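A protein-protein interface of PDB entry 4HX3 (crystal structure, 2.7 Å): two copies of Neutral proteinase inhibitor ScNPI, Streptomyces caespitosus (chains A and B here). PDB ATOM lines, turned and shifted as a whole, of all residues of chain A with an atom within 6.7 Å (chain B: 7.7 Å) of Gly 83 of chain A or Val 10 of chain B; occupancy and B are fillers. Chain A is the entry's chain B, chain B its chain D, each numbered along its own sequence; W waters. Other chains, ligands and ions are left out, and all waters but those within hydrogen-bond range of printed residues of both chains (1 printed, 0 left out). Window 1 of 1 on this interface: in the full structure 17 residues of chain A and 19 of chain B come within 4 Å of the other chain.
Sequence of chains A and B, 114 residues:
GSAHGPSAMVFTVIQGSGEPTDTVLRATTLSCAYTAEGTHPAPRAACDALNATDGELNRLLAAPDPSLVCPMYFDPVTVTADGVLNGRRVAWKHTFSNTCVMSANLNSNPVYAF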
ATOM      1  N   ALA A   8      17.486  12.023   1.663  1.00  0.00           N
ATOM      2  CA  ALA A   8      16.600  13.061   1.113  1.00  0.00           C
ATOM      3  C   ALA A   8      15.198  12.672   1.526  1.00  0.00           C
ATOM      4  O   ALA A   8      14.673  11.696   1.014  1.00  0.00           O
ATOM      5  CB  ALA A   8      16.758  13.163  -0.400  1.00  0.00           C
ATOM      6  N   MET A   9      14.651  13.346   2.546  1.00  0.00           N
ATOM      7  CA  MET A   9      13.373  12.934   3.154  1.00  0.00           C
ATOM      8  C   MET A   9      12.355  14.013   3.266  1.00  0.00           C
ATOM      9  O   MET A   9      12.719  15.178   3.335  1.00  0.00           O
ATOM     10  CB  MET A   9      13.613  12.451   4.593  1.00  0.00           C
ATOM     11  CG  MET A   9      14.636  11.337   4.737  1.00  0.00           C
ATOM     12  SD  MET A   9      13.881   9.725   4.487  1.00  0.00           S
ATOM     13  CE  MET A   9      12.842   9.617   5.887  1.00  0.00           C
ATOM     14  N   VAL A  10      11.081  13.605   3.372  1.00  0.00           N
ATOM     15  CA  VAL A  10       9.909  14.424   3.691  1.00  0.00           C
ATOM     16  C   VAL A  10       9.357  13.897   5.019  1.00  0.00           C
ATOM     17  O   VAL A  10       9.120  12.688   5.149  1.00  0.00           O
ATOM     18  CB  VAL A  10       8.775  14.487   2.630  1.00  0.00           C
ATOM     19  CG1 VAL A  10       7.681  15.471   3.047  1.00  0.00           C
ATOM     20  CG2 VAL A  10       9.294  14.840   1.268  1.00  0.00           C
ATOM     21  N   THR A  29      11.108  19.266   4.457  1.00  0.00           N
ATOM     22  CA  THR A  29      12.060  18.481   3.686  1.00  0.00           C
ATOM     23  C   THR A  29      13.415  18.578   4.332  1.00  0.00           C
ATOM     24  O   THR A  29      13.740  19.585   4.977  1.00  0.00           O
ATOM     25  CB  THR A  29      12.115  18.920   2.192  1.00  0.00           C
ATOM     26  OG1 THR A  29      12.606  20.263   2.076  1.00  0.00           O
ATOM     27  CG2 THR A  29      10.772  18.788   1.477  1.00  0.00           C
ATOM     28  N   LEU A  30      14.207  17.532   4.175  1.00  0.00           N
ATOM     29  CA  LEU A  30      15.559  17.455   4.752  1.00  0.00           C
ATOM     30  C   LEU A  30      16.447  16.639   3.863  1.00  0.00           C
ATOM     31  O   LEU A  30      16.045  15.580   3.378  1.00  0.00           O
ATOM     32  CB  LEU A  30      15.506  16.832   6.159  1.00  0.00           C
ATOM     33  CG  LEU A  30      16.758  16.827   7.018  1.00  0.00           C
ATOM     34  CD1 LEU A  30      17.237  18.278   7.365  1.00  0.00           C
ATOM     35  CD2 LEU A  30      16.481  16.016   8.269  1.00  0.00           C
ATOM     36  N   ALA A  81       7.525   9.717   7.607  1.00  0.00           N
ATOM     37  CA  ALA A  81       8.867   9.911   7.059  1.00  0.00           C
ATOM     38  C   ALA A  81       8.958   9.087   5.786  1.00  0.00           C
ATOM     39  O   ALA A  81       8.710   7.877   5.815  1.00  0.00           O
ATOM     40  CB  ALA A  81       9.923   9.501   8.069  1.00  0.00           C
ATOM     41  N   ASP A  82       9.187   9.759   4.647  1.00  0.00           N
ATOM     42  CA  ASP A  82       9.259   9.136   3.324  1.00  0.00           C
ATOM     43  C   ASP A  82      10.412   9.708   2.550  1.00  0.00           C
ATOM     44  O   ASP A  82      10.694  10.897   2.666  1.00  0.00           O
ATOM     45  CB  ASP A  82       7.959   9.361   2.541  1.00  0.00           C
ATOM     46  CG  ASP A  82       6.712   8.799   3.187  1.00  0.00           C
ATOM     47  OD1 ASP A  82       6.410   7.591   2.960  1.00  0.00           O
ATOM     48  OD2 ASP A  82       5.992   9.578   3.861  1.00  0.00           O
ATOM     49  N   GLY A  83      11.093   8.865   1.797  1.00  0.00           N
ATOM     50  CA  GLY A  83      12.214   9.299   0.991  1.00  0.00           C
ATOM     51  C   GLY A  83      13.353   8.321   0.972  1.00  0.00           C
ATOM     52  O   GLY A  83      13.148   7.105   0.981  1.00  0.00           O
ATOM     53  N   VAL A  84      14.567   8.871   0.901  1.00  0.00           N
ATOM     54  CA  VAL A  84      15.816   8.129   0.836  1.00  0.00           C
ATOM     55  C   VAL A  84      16.495   8.289   2.154  1.00  0.00           C
ATOM     56  O   VAL A  84      16.719   9.409   2.585  1.00  0.00           O
ATOM     57  CB  VAL A  84      16.683   8.630  -0.321  1.00  0.00           C
ATOM     58  CG1 VAL A  84      18.055   7.964  -0.303  1.00  0.00           C
ATOM     59  CG2 VAL A  84      15.979   8.439  -1.659  1.00  0.00           C
ATOM     60  N   LEU A  85      16.782   7.183   2.816  1.00  0.00           N
ATOM     61  CA  LEU A  85      17.473   7.154   4.101  1.00  0.00           C
ATOM     62  C   LEU A  85      18.684   6.240   3.956  1.00  0.00           C
ATOM     63  O   LEU A  85      18.539   5.052   3.651  1.00  0.00           O
ATOM     64  CB  LEU A  85      16.522   6.679   5.213  1.00  0.00           C
ATOM     65  CG  LEU A  85      17.087   6.578   6.615  1.00  0.00           C
ATOM     66  CD1 LEU A  85      17.378   7.929   7.176  1.00  0.00           C
ATOM     67  CD2 LEU A  85      16.134   5.856   7.489  1.00  0.00           C
ATOM     68  N   ARG A  88      18.807   4.275   0.608  1.00  0.00           N
ATOM     69  CA  ARG A  88      17.746   3.314   0.352  1.00  0.00           C
ATOM     70  C   ARG A  88      16.411   3.968   0.633  1.00  0.00           C
ATOM     71  O   ARG A  88      16.274   4.762   1.570  1.00  0.00           O
ATOM     72  CB  ARG A  88      17.939   2.021   1.166  1.00  0.00           C
ATOM     73  CG  ARG A  88      19.231   1.232   0.816  1.00  0.00           C
ATOM     74  CD  ARG A  88      19.212   0.537  -0.529  1.00  0.00           C
ATOM     75  NE  ARG A  88      20.441  -0.221  -0.783  1.00  0.00           N
ATOM     76  CZ  ARG A  88      21.483   0.228  -1.482  1.00  0.00           C
ATOM     77  NH1 ARG A  88      21.479   1.461  -1.978  1.00  0.00           N
ATOM     78  NH2 ARG A  88      22.539  -0.553  -1.688  1.00  0.00           N
ATOM     79  N   ARG A  89      15.435   3.673  -0.241  1.00  0.00           N
ATOM     80  CA  ARG A  89      14.081   4.220  -0.211  1.00  0.00           C
ATOM     81  C   ARG A  89      13.349   3.643   0.993  1.00  0.00           C
ATOM     82  O   ARG A  89      13.438   2.452   1.258  1.00  0.00           O
ATOM     83  CB  ARG A  89      13.369   3.931  -1.544  1.00  0.00           C
ATOM     84  CG  ARG A  89      12.200   4.857  -1.817  1.00  0.00           C
ATOM     85  CD  ARG A  89      11.482   4.514  -3.097  1.00  0.00           C
ATOM     86  NE  ARG A  89      10.138   5.084  -3.117  1.00  0.00           N
ATOM     87  CZ  ARG A  89       9.023   4.362  -3.101  1.00  0.00           C
ATOM     88  NH1 ARG A  89       9.082   3.036  -3.084  1.00  0.00           N
ATOM     89  NH2 ARG A  89       7.837   4.960  -3.122  1.00  0.00           N
ATOM     90  N   VAL A  90      12.713   4.507   1.786  1.00  0.00           N
ATOM     91  CA  VAL A  90      11.996   4.117   3.010  1.00  0.00           C
ATOM     92  C   VAL A  90      10.648   4.829   3.125  1.00  0.00           C
ATOM     93  O   VAL A  90      10.431   5.876   2.497  1.00  0.00           O
ATOM     94  CB  VAL A  90      12.807   4.341   4.310  1.00  0.00           C
ATOM     95  CG1 VAL A  90      14.142   3.608   4.285  1.00  0.00           C
ATOM     96  CG2 VAL A  90      12.957   5.821   4.629  1.00  0.00           C
ATOM     97  N   ALA A  91       9.752   4.240   3.944  1.00  0.00           N
ATOM     98  CA  ALA A  91       8.411   4.742   4.268  1.00  0.00           C
ATOM     99  C   ALA A  91       8.059   4.273   5.653  1.00  0.00           C
ATOM    100  O   ALA A  91       8.083   3.070   5.946  1.00  0.00           O
ATOM    101  CB  ALA A  91       7.369   4.275   3.256  1.00  0.00           C
ATOM    102  N   ALA B   8       5.329  19.634  -0.500  1.00  0.00           N
ATOM    103  CA  ALA B   8       6.653  19.299   0.011  1.00  0.00           C
ATOM    104  C   ALA B   8       6.911  17.875  -0.386  1.00  0.00           C
ATOM    105  O   ALA B   8       6.304  16.959   0.173  1.00  0.00           O
ATOM    106  CB  ALA B   8       6.690  19.468   1.524  1.00  0.00           C
ATOM    107  N   MET B   9       7.742  17.685  -1.421  1.00  0.00           N
ATOM    108  CA  MET B   9       7.968  16.384  -2.033  1.00  0.00           C
ATOM    109  C   MET B   9       9.397  15.953  -2.088  1.00  0.00           C
ATOM    110  O   MET B   9      10.308  16.784  -2.107  1.00  0.00           O
ATOM    111  CB  MET B   9       7.473  16.408  -3.494  1.00  0.00           C
ATOM    112  CG  MET B   9       5.990  16.692  -3.692  1.00  0.00           C
ATOM    113  SD  MET B   9       4.943  15.275  -3.331  1.00  0.00           S
ATOM    114  CE  MET B   9       4.876  14.472  -4.909  1.00  0.00           C
ATOM    115  N   VAL B  10       9.581  14.612  -2.167  1.00  0.00           N
ATOM    116  CA  VAL B  10      10.842  13.936  -2.426  1.00  0.00           C
ATOM    117  C   VAL B  10      10.638  13.097  -3.701  1.00  0.00           C
ATOM    118  O   VAL B  10       9.693  12.309  -3.790  1.00  0.00           O
ATOM    119  CB  VAL B  10      11.423  13.127  -1.245  1.00  0.00           C
ATOM    120  CG1 VAL B  10      10.482  12.030  -0.793  1.00  0.00           C
ATOM    121  CG2 VAL B  10      12.810  12.557  -1.592  1.00  0.00           C
ATOM    122  N   PHE B  11      11.480  13.345  -4.719  1.00  0.00           N
ATOM    123  CA  PHE B  11      11.451  12.634  -6.004  1.00  0.00           C
ATOM    124  C   PHE B  11      12.689  11.791  -6.106  1.00  0.00           C
ATOM    125  O   PHE B  11      13.736  12.201  -5.586  1.00  0.00           O
ATOM    126  CB  PHE B  11      11.370  13.621  -7.156  1.00  0.00           C
ATOM    127  CG  PHE B  11      10.170  14.524  -7.057  1.00  0.00           C
ATOM    128  CD1 PHE B  11       8.909  14.084  -7.465  1.00  0.00           C
ATOM    129  CD2 PHE B  11      10.291  15.814  -6.562  1.00  0.00           C
ATOM    130  CE1 PHE B  11       7.798  14.908  -7.364  1.00  0.00           C
ATOM    131  CE2 PHE B  11       9.171  16.656  -6.469  1.00  0.00           C
ATOM    132  CZ  PHE B  11       7.934  16.195  -6.871  1.00  0.00           C
ATOM    133  N   THR B  12      12.559  10.570  -6.635  1.00  0.00           N
ATOM    134  CA  THR B  12      13.697   9.652  -6.806  1.00  0.00           C
ATOM    135  C   THR B  12      13.646   8.902  -8.158  1.00  0.00           C
ATOM    136  O   THR B  12      12.593   8.798  -8.795  1.00  0.00           O
ATOM    137  CB  THR B  12      13.837   8.587  -5.671  1.00  0.00           C
ATOM    138  OG1 THR B  12      13.183   7.385  -6.046  1.00  0.00           O
ATOM    139  CG2 THR B  12      13.376   9.046  -4.308  1.00  0.00           C
ATOM    140  N   ILE B  14      15.295   5.142  -9.249  1.00  0.00           N
ATOM    141  CA  ILE B  14      15.905   3.970  -8.658  1.00  0.00           C
ATOM    142  C   ILE B  14      16.265   2.944  -9.711  1.00  0.00           C
ATOM    143  O   ILE B  14      15.506   2.736 -10.662  1.00  0.00           O
ATOM    144  CB  ILE B  14      14.929   3.408  -7.594  1.00  0.00           C
ATOM    145  CG1 ILE B  14      15.138   4.115  -6.269  1.00  0.00           C
ATOM    146  CG2 ILE B  14      15.055   1.920  -7.395  1.00  0.00           C
ATOM    147  CD1 ILE B  14      13.890   4.451  -5.560  1.00  0.00           C
ATOM    148  N   VAL B  24      19.652   3.851  -5.290  1.00  0.00           N
ATOM    149  CA  VAL B  24      19.017   5.120  -5.651  1.00  0.00           C
ATOM    150  C   VAL B  24      20.024   5.813  -6.562  1.00  0.00           C
ATOM    151  O   VAL B  24      21.182   6.047  -6.163  1.00  0.00           O
ATOM    152  CB  VAL B  24      18.605   5.969  -4.398  1.00  0.00           C
ATOM    153  CG1 VAL B  24      18.180   7.374  -4.773  1.00  0.00           C
ATOM    154  CG2 VAL B  24      17.515   5.283  -3.574  1.00  0.00           C
ATOM    155  N   ARG B  26      19.312   8.807  -8.317  1.00  0.00           N
ATOM    156  CA  ARG B  26      19.238  10.236  -8.025  1.00  0.00           C
ATOM    157  C   ARG B  26      18.029  10.519  -7.191  1.00  0.00           C
ATOM    158  O   ARG B  26      17.092   9.758  -7.209  1.00  0.00           O
ATOM    159  CB  ARG B  26      19.267  11.121  -9.288  1.00  0.00           C
ATOM    160  CG  ARG B  26      18.475  10.653 -10.522  1.00  0.00           C
ATOM    161  CD  ARG B  26      18.859  11.485 -11.744  1.00  0.00           C
ATOM    162  NE  ARG B  26      18.140  11.135 -12.975  1.00  0.00           N
ATOM    163  CZ  ARG B  26      17.057  11.773 -13.421  1.00  0.00           C
ATOM    164  NH1 ARG B  26      16.538  12.778 -12.730  1.00  0.00           N
ATOM    165  NH2 ARG B  26      16.470  11.390 -14.548  1.00  0.00           N
ATOM    166  N   ALA B  27      18.096  11.553  -6.374  1.00  0.00           N
ATOM    167  CA  ALA B  27      16.991  12.024  -5.527  1.00  0.00           C
ATOM    168  C   ALA B  27      17.129  13.514  -5.228  1.00  0.00           C
ATOM    169  O   ALA B  27      18.221  14.070  -5.248  1.00  0.00           O
ATOM    170  CB  ALA B  27      16.910  11.234  -4.228  1.00  0.00           C
ATOM    171  N   THR B  28      15.994  14.178  -5.009  1.00  0.00           N
ATOM    172  CA  THR B  28      15.948  15.624  -4.707  1.00  0.00           C
ATOM    173  C   THR B  28      14.696  15.929  -3.909  1.00  0.00           C
ATOM    174  O   THR B  28      13.756  15.125  -3.880  1.00  0.00           O
ATOM    175  CB  THR B  28      16.034  16.445  -6.010  1.00  0.00           C
ATOM    176  OG1 THR B  28      16.492  17.769  -5.739  1.00  0.00           O
ATOM    177  CG2 THR B  28      14.754  16.412  -6.824  1.00  0.00           C
ATOM    178  N   THR B  29      14.690  17.098  -3.275  1.00  0.00           N
ATOM    179  CA  THR B  29      13.552  17.619  -2.505  1.00  0.00           C
ATOM    180  C   THR B  29      13.012  18.870  -3.210  1.00  0.00           C
ATOM    181  O   THR B  29      13.771  19.607  -3.849  1.00  0.00           O
ATOM    182  CB  THR B  29      13.915  17.865  -1.030  1.00  0.00           C
ATOM    183  OG1 THR B  29      14.870  18.913  -0.933  1.00  0.00           O
ATOM    184  CG2 THR B  29      14.430  16.602  -0.340  1.00  0.00           C
ATOM    185  N   LEU B  30      11.702  19.088  -3.086  1.00  0.00           N
ATOM    186  CA  LEU B  30      11.008  20.241  -3.644  1.00  0.00           C
ATOM    187  C   LEU B  30       9.928  20.726  -2.693  1.00  0.00           C
ATOM    188  O   LEU B  30       9.212  19.917  -2.113  1.00  0.00           O
ATOM    189  CB  LEU B  30      10.412  19.873  -4.997  1.00  0.00           C
ATOM    190  CG  LEU B  30       9.831  20.995  -5.849  1.00  0.00           C
ATOM    191  CD1 LEU B  30      10.926  22.039  -6.267  1.00  0.00           C
ATOM    192  CD2 LEU B  30       9.164  20.399  -7.070  1.00  0.00           C
ATOM    193  N   SER B  31       9.827  22.045  -2.520  1.00  0.00           N
ATOM    194  CA  SER B  31       8.816  22.662  -1.660  1.00  0.00           C
ATOM    195  C   SER B  31       8.166  23.852  -2.391  1.00  0.00           C
ATOM    196  O   SER B  31       8.879  24.713  -2.902  1.00  0.00           O
ATOM    197  CB  SER B  31       9.434  23.085  -0.332  1.00  0.00           C
ATOM    198  OG  SER B  31       8.446  23.562   0.565  1.00  0.00           O
ATOM    199  N   THR B  39      16.111  21.149  -2.829  1.00  0.00           N
ATOM    200  CA  THR B  39      17.447  20.825  -3.351  1.00  0.00           C
ATOM    201  C   THR B  39      17.381  20.647  -4.878  1.00  0.00           C
ATOM    202  O   THR B  39      18.396  20.373  -5.513  1.00  0.00           O
ATOM    203  CB  THR B  39      18.053  19.614  -2.650  1.00  0.00           C
ATOM    204  OG1 THR B  39      17.199  18.479  -2.829  1.00  0.00           O
ATOM    205  CG2 THR B  39      18.334  19.876  -1.186  1.00  0.00           C
ATOM    206  N   THR B  80       9.828   7.735  -8.576  1.00  0.00           N
ATOM    207  CA  THR B  80       8.924   7.825  -7.411  1.00  0.00           C
ATOM    208  C   THR B  80       8.712   9.288  -6.999  1.00  0.00           C
ATOM    209  O   THR B  80       9.524  10.154  -7.338  1.00  0.00           O
ATOM    210  CB  THR B  80       9.421   7.005  -6.199  1.00  0.00           C
ATOM    211  OG1 THR B  80      10.535   7.679  -5.617  1.00  0.00           O
ATOM    212  CG2 THR B  80       9.761   5.560  -6.540  1.00  0.00           C
ATOM    213  N   ALA B  81       7.624   9.534  -6.242  1.00  0.00           N
ATOM    214  CA  ALA B  81       7.220  10.835  -5.699  1.00  0.00           C
ATOM    215  C   ALA B  81       6.464  10.593  -4.404  1.00  0.00           C
ATOM    216  O   ALA B  81       5.510   9.811  -4.377  1.00  0.00           O
ATOM    217  CB  ALA B  81       6.369  11.587  -6.708  1.00  0.00           C
ATOM    218  N   ASP B  82       6.958  11.157  -3.314  1.00  0.00           N
ATOM    219  CA  ASP B  82       6.387  10.971  -1.974  1.00  0.00           C
ATOM    220  C   ASP B  82       6.369  12.288  -1.243  1.00  0.00           C
ATOM    221  O   ASP B  82       7.310  13.075  -1.376  1.00  0.00           O
ATOM    222  CB  ASP B  82       7.209   9.936  -1.162  1.00  0.00           C
ATOM    223  CG  ASP B  82       7.244   8.546  -1.750  1.00  0.00           C
ATOM    224  OD1 ASP B  82       6.313   7.763  -1.478  1.00  0.00           O
ATOM    225  OD2 ASP B  82       8.236   8.217  -2.421  1.00  0.00           O
ATOM    226  N   GLY B  83       5.332  12.502  -0.445  1.00  0.00           N
ATOM    227  CA  GLY B  83       5.215  13.721   0.341  1.00  0.00           C
ATOM    228  C   GLY B  83       3.831  14.322   0.345  1.00  0.00           C
ATOM    229  O   GLY B  83       2.819  13.616   0.334  1.00  0.00           O
ATOM    230  N   VAL B  84       3.804  15.644   0.372  1.00  0.00           N
ATOM    231  CA  VAL B  84       2.581  16.437   0.445  1.00  0.00           C
ATOM    232  C   VAL B  84       2.371  17.104  -0.872  1.00  0.00           C
ATOM    233  O   VAL B  84       3.244  17.825  -1.329  1.00  0.00           O
ATOM    234  CB  VAL B  84       2.659  17.462   1.599  1.00  0.00           C
ATOM    235  CG1 VAL B  84       1.427  18.365   1.636  1.00  0.00           C
ATOM    236  CG2 VAL B  84       2.833  16.756   2.931  1.00  0.00           C
ATOM    237  N   VAL B  90       0.682  12.012  -0.383  1.00  0.00           N
ATOM    238  CA  VAL B  90       0.646  11.165  -1.582  1.00  0.00           C
ATOM    239  C   VAL B  90       1.901  10.282  -1.687  1.00  0.00           C
ATOM    240  O   VAL B  90       2.951  10.610  -1.115  1.00  0.00           O
ATOM    241  CB  VAL B  90       0.448  11.958  -2.897  1.00  0.00           C
ATOM    242  CG1 VAL B  90      -0.818  12.800  -2.879  1.00  0.00           C
ATOM    243  CG2 VAL B  90       1.680  12.771  -3.258  1.00  0.00           C
ATOM    244  N   TRP B  92       3.505   7.846  -5.026  1.00  0.00           N
ATOM    245  CA  TRP B  92       3.406   7.439  -6.412  1.00  0.00           C
ATOM    246  C   TRP B  92       4.721   6.884  -6.910  1.00  0.00           C
ATOM    247  O   TRP B  92       5.782   7.329  -6.487  1.00  0.00           O
ATOM    248  CB  TRP B  92       2.986   8.660  -7.237  1.00  0.00           C
ATOM    249  CG  TRP B  92       2.908   8.463  -8.718  1.00  0.00           C
ATOM    250  CD1 TRP B  92       1.821   8.070  -9.437  1.00  0.00           C
ATOM    251  CD2 TRP B  92       3.931   8.771  -9.670  1.00  0.00           C
ATOM    252  NE1 TRP B  92       2.115   8.071 -10.776  1.00  0.00           N
ATOM    253  CE2 TRP B  92       3.396   8.524 -10.949  1.00  0.00           C
ATOM    254  CE3 TRP B  92       5.256   9.236  -9.567  1.00  0.00           C
ATOM    255  CZ2 TRP B  92       4.124   8.739 -12.107  1.00  0.00           C
ATOM    256  CZ3 TRP B  92       5.978   9.450 -10.722  1.00  0.00           C
ATOM    257  CH2 TRP B  92       5.409   9.200 -11.973  1.00  0.00           C
ATOM    258  N   TYR B 112      11.530  15.916 -13.180  1.00  0.00           N
ATOM    259  CA  TYR B 112      12.643  14.948 -13.139  1.00  0.00           C
ATOM    260  C   TYR B 112      13.933  15.465 -13.778  1.00  0.00           C
ATOM    261  O   TYR B 112      14.881  14.702 -13.969  1.00  0.00           O
ATOM    262  CB  TYR B 112      12.229  13.590 -13.711  1.00  0.00           C
ATOM    263  CG  TYR B 112      11.334  12.864 -12.730  1.00  0.00           C
ATOM    264  CD1 TYR B 112      11.871  12.003 -11.770  1.00  0.00           C
ATOM    265  CD2 TYR B 112       9.959  13.110 -12.692  1.00  0.00           C
ATOM    266  CE1 TYR B 112      11.062  11.399 -10.804  1.00  0.00           C
ATOM    267  CE2 TYR B 112       9.140  12.496 -11.742  1.00  0.00           C
ATOM    268  CZ  TYR B 112       9.697  11.644 -10.799  1.00  0.00           C
ATOM    269  OH  TYR B 112       8.886  11.015  -9.886  1.00  0.00           O
ATOM    270  N   PHE B 114      16.629  16.643 -12.630  1.00  0.00           N
ATOM    271  CA  PHE B 114      17.562  16.745 -11.506  1.00  0.00           C
ATOM    272  C   PHE B 114      18.665  15.686 -11.643  1.00  0.00           C
ATOM    273  O   PHE B 114      18.464  14.736 -12.433  1.00  0.00           O
ATOM    274  CB  PHE B 114      16.831  16.638 -10.143  1.00  0.00           C
ATOM    275  CG  PHE B 114      16.087  15.349  -9.858  1.00  0.00           C
ATOM    276  CD1 PHE B 114      16.739  14.264  -9.267  1.00  0.00           C
ATOM    277  CD2 PHE B 114      14.728  15.241 -10.122  1.00  0.00           C
ATOM    278  CE1 PHE B 114      16.048  13.093  -8.974  1.00  0.00           C
ATOM    279  CE2 PHE B 114      14.028  14.073  -9.804  1.00  0.00           C
ATOM    280  CZ  PHE B 114      14.691  13.006  -9.244  1.00  0.00           C
ATOM    281  OXT PHE B 114      19.728  15.819 -10.982  1.00  0.00           O
HETATM  282  O   HOH W   1      22.073   3.893  -3.076  1.00  0.00           O
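Among the printed residues, pairs that only touch across the chains: Ala 8 of chain A with Val 10 of chain B (3.3 Å), Val 10 of chain A with Ala 8 of chain B (3.5 Å), Val 10 of chain A with Met 9 of chain B (3.5 Å), Val 10 of chain A with Val 10 of chain B (3.5 Å), Val 10 of chain A with Asp 82 of chain B (3.7 Å), Thr 29 of chain A with Thr 29 of chain B (3.8 Å), Asp 82 of chain A with Val 10 of chain B (3.6 Å), Asp 82 of chain A with Asp 82 of chain B (3.8 Å), Gly 83 of chain A with Val 10 of chain B (3.7 Å), Val 84 of chain A with Thr 12 of chain B (3.8 Å), Val 84 of chain A with Val 24 of chain B (3.96 Å), Val 84 of chain A with Ala 27 of chain B (3.9 Å), Arg 89 of chain A with Ile 14 of chain B (3.4 Å) and Arg 89 of chain A with Thr 80 of chain B (3.5 Å).
Of the 14 printed residues of chain A, 7 touch a printed residue of chain B. Printed residues of chain A that touch a printed residue of chain B: Ala 8, Val 10, Thr 29, Asp 82, Gly 83, Val 84 and Arg 89. Hydrophobic or aromatic side chains of chain B within 4 Å of the printed part of chain A: Val 10, Ile 14, Val 24 and Ala 27. Among the printed residues, Asp or Glu carboxylates within 4 Å of a Lys or Arg side-chain nitrogen of the other chain: Arg 89 of chain A with Asp 82 of chain B (3.4 Å).
The guanidinium group (NH2) of Arg 89 of chain A lies within salt-bridge range of the side-chain carboxylate (OD2) of Asp 82 of chain B.
Water W1 bridges the guanidinium group of Arg 88 of chain A and the backbone NH of Val 24 of chain B.
Ala 8 of chain A touches Val 10 of chain B, and with the chains exchanged Val 10 of chain A touches Ala 8 of chain B. Val 10 of chain A touches Met 9 of chain B, but with the chains exchanged Met 9 of chain A does not touch Val 10 of chain B (4.6 Å). Val 10 of chain A touches its own counterpart, Val 10 of chain B. Gly 83 of chain A touches Val 10 of chain B, but with the chains exchanged Val 10 of chain A does not touch Gly 83 of chain B (4.1 Å). Of the 15 pairs that touch across the chains among the printed residues, 7 have their exchanged pair printed and touching as well.
Gly 83 of chain A touches just one residue of chain B: Val 10. Val 10 of chain B touches just these residues of chain A: Ala 8, Val 10, Asp 82 and Gly 83. Of the printed residues of chain B, Asp 82 of chain A touches Val 10 (3.6 Å) and Asp 82 (3.8 Å). Printed residues of chain A within 4 Å of Val 24 of chain B: Val 84 (3.96 Å). Printed residues of chain A within 4 Å of Ile 14 of chain B: Arg 89. Of the printed residues of chain B, Val 10 of chain A touches Ala 8, Met 9, Val 10 and Asp 82. Phe 114 of chain B touches none of the printed residues of chain A. The nearest residue of chain B that does not touch Gly 83 of chain A is Asp 82 of chain B (5.0 Å). The nearest residue of chain A that does not touch Val 10 of chain B is Met 9 of chain A (4.6 Å).
SD of Met 9 of chain A sits at hydrogen-bond distance from N of Val 84 of chain A. The backbone NH (N) of Val 90 of chain A is in hydrogen-bond range of the backbone carbonyl oxygen (O) of Gly 83 of chain A (2.8 Å). The backbone NH of Val 84 of chain B sits at hydrogen-bond distance from the backbone carbonyl oxygen of Ala 8 of chain B, 2.8 Å away. The backbone NH (N) of Val 10 of chain B is in hydrogen-bond range of the backbone carbonyl oxygen (O) of Asp 82 of chain B, 2.9 Å away. The backbone NH (N) of Thr 29 of chain B lies within hydrogen-bond range of the side-chain hydroxyl (OG1) of Thr 39 of chain B. O of Thr 80 of chain B lies within hydrogen-bond range of OH of Tyr 112 of chain B (2.8 Å).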
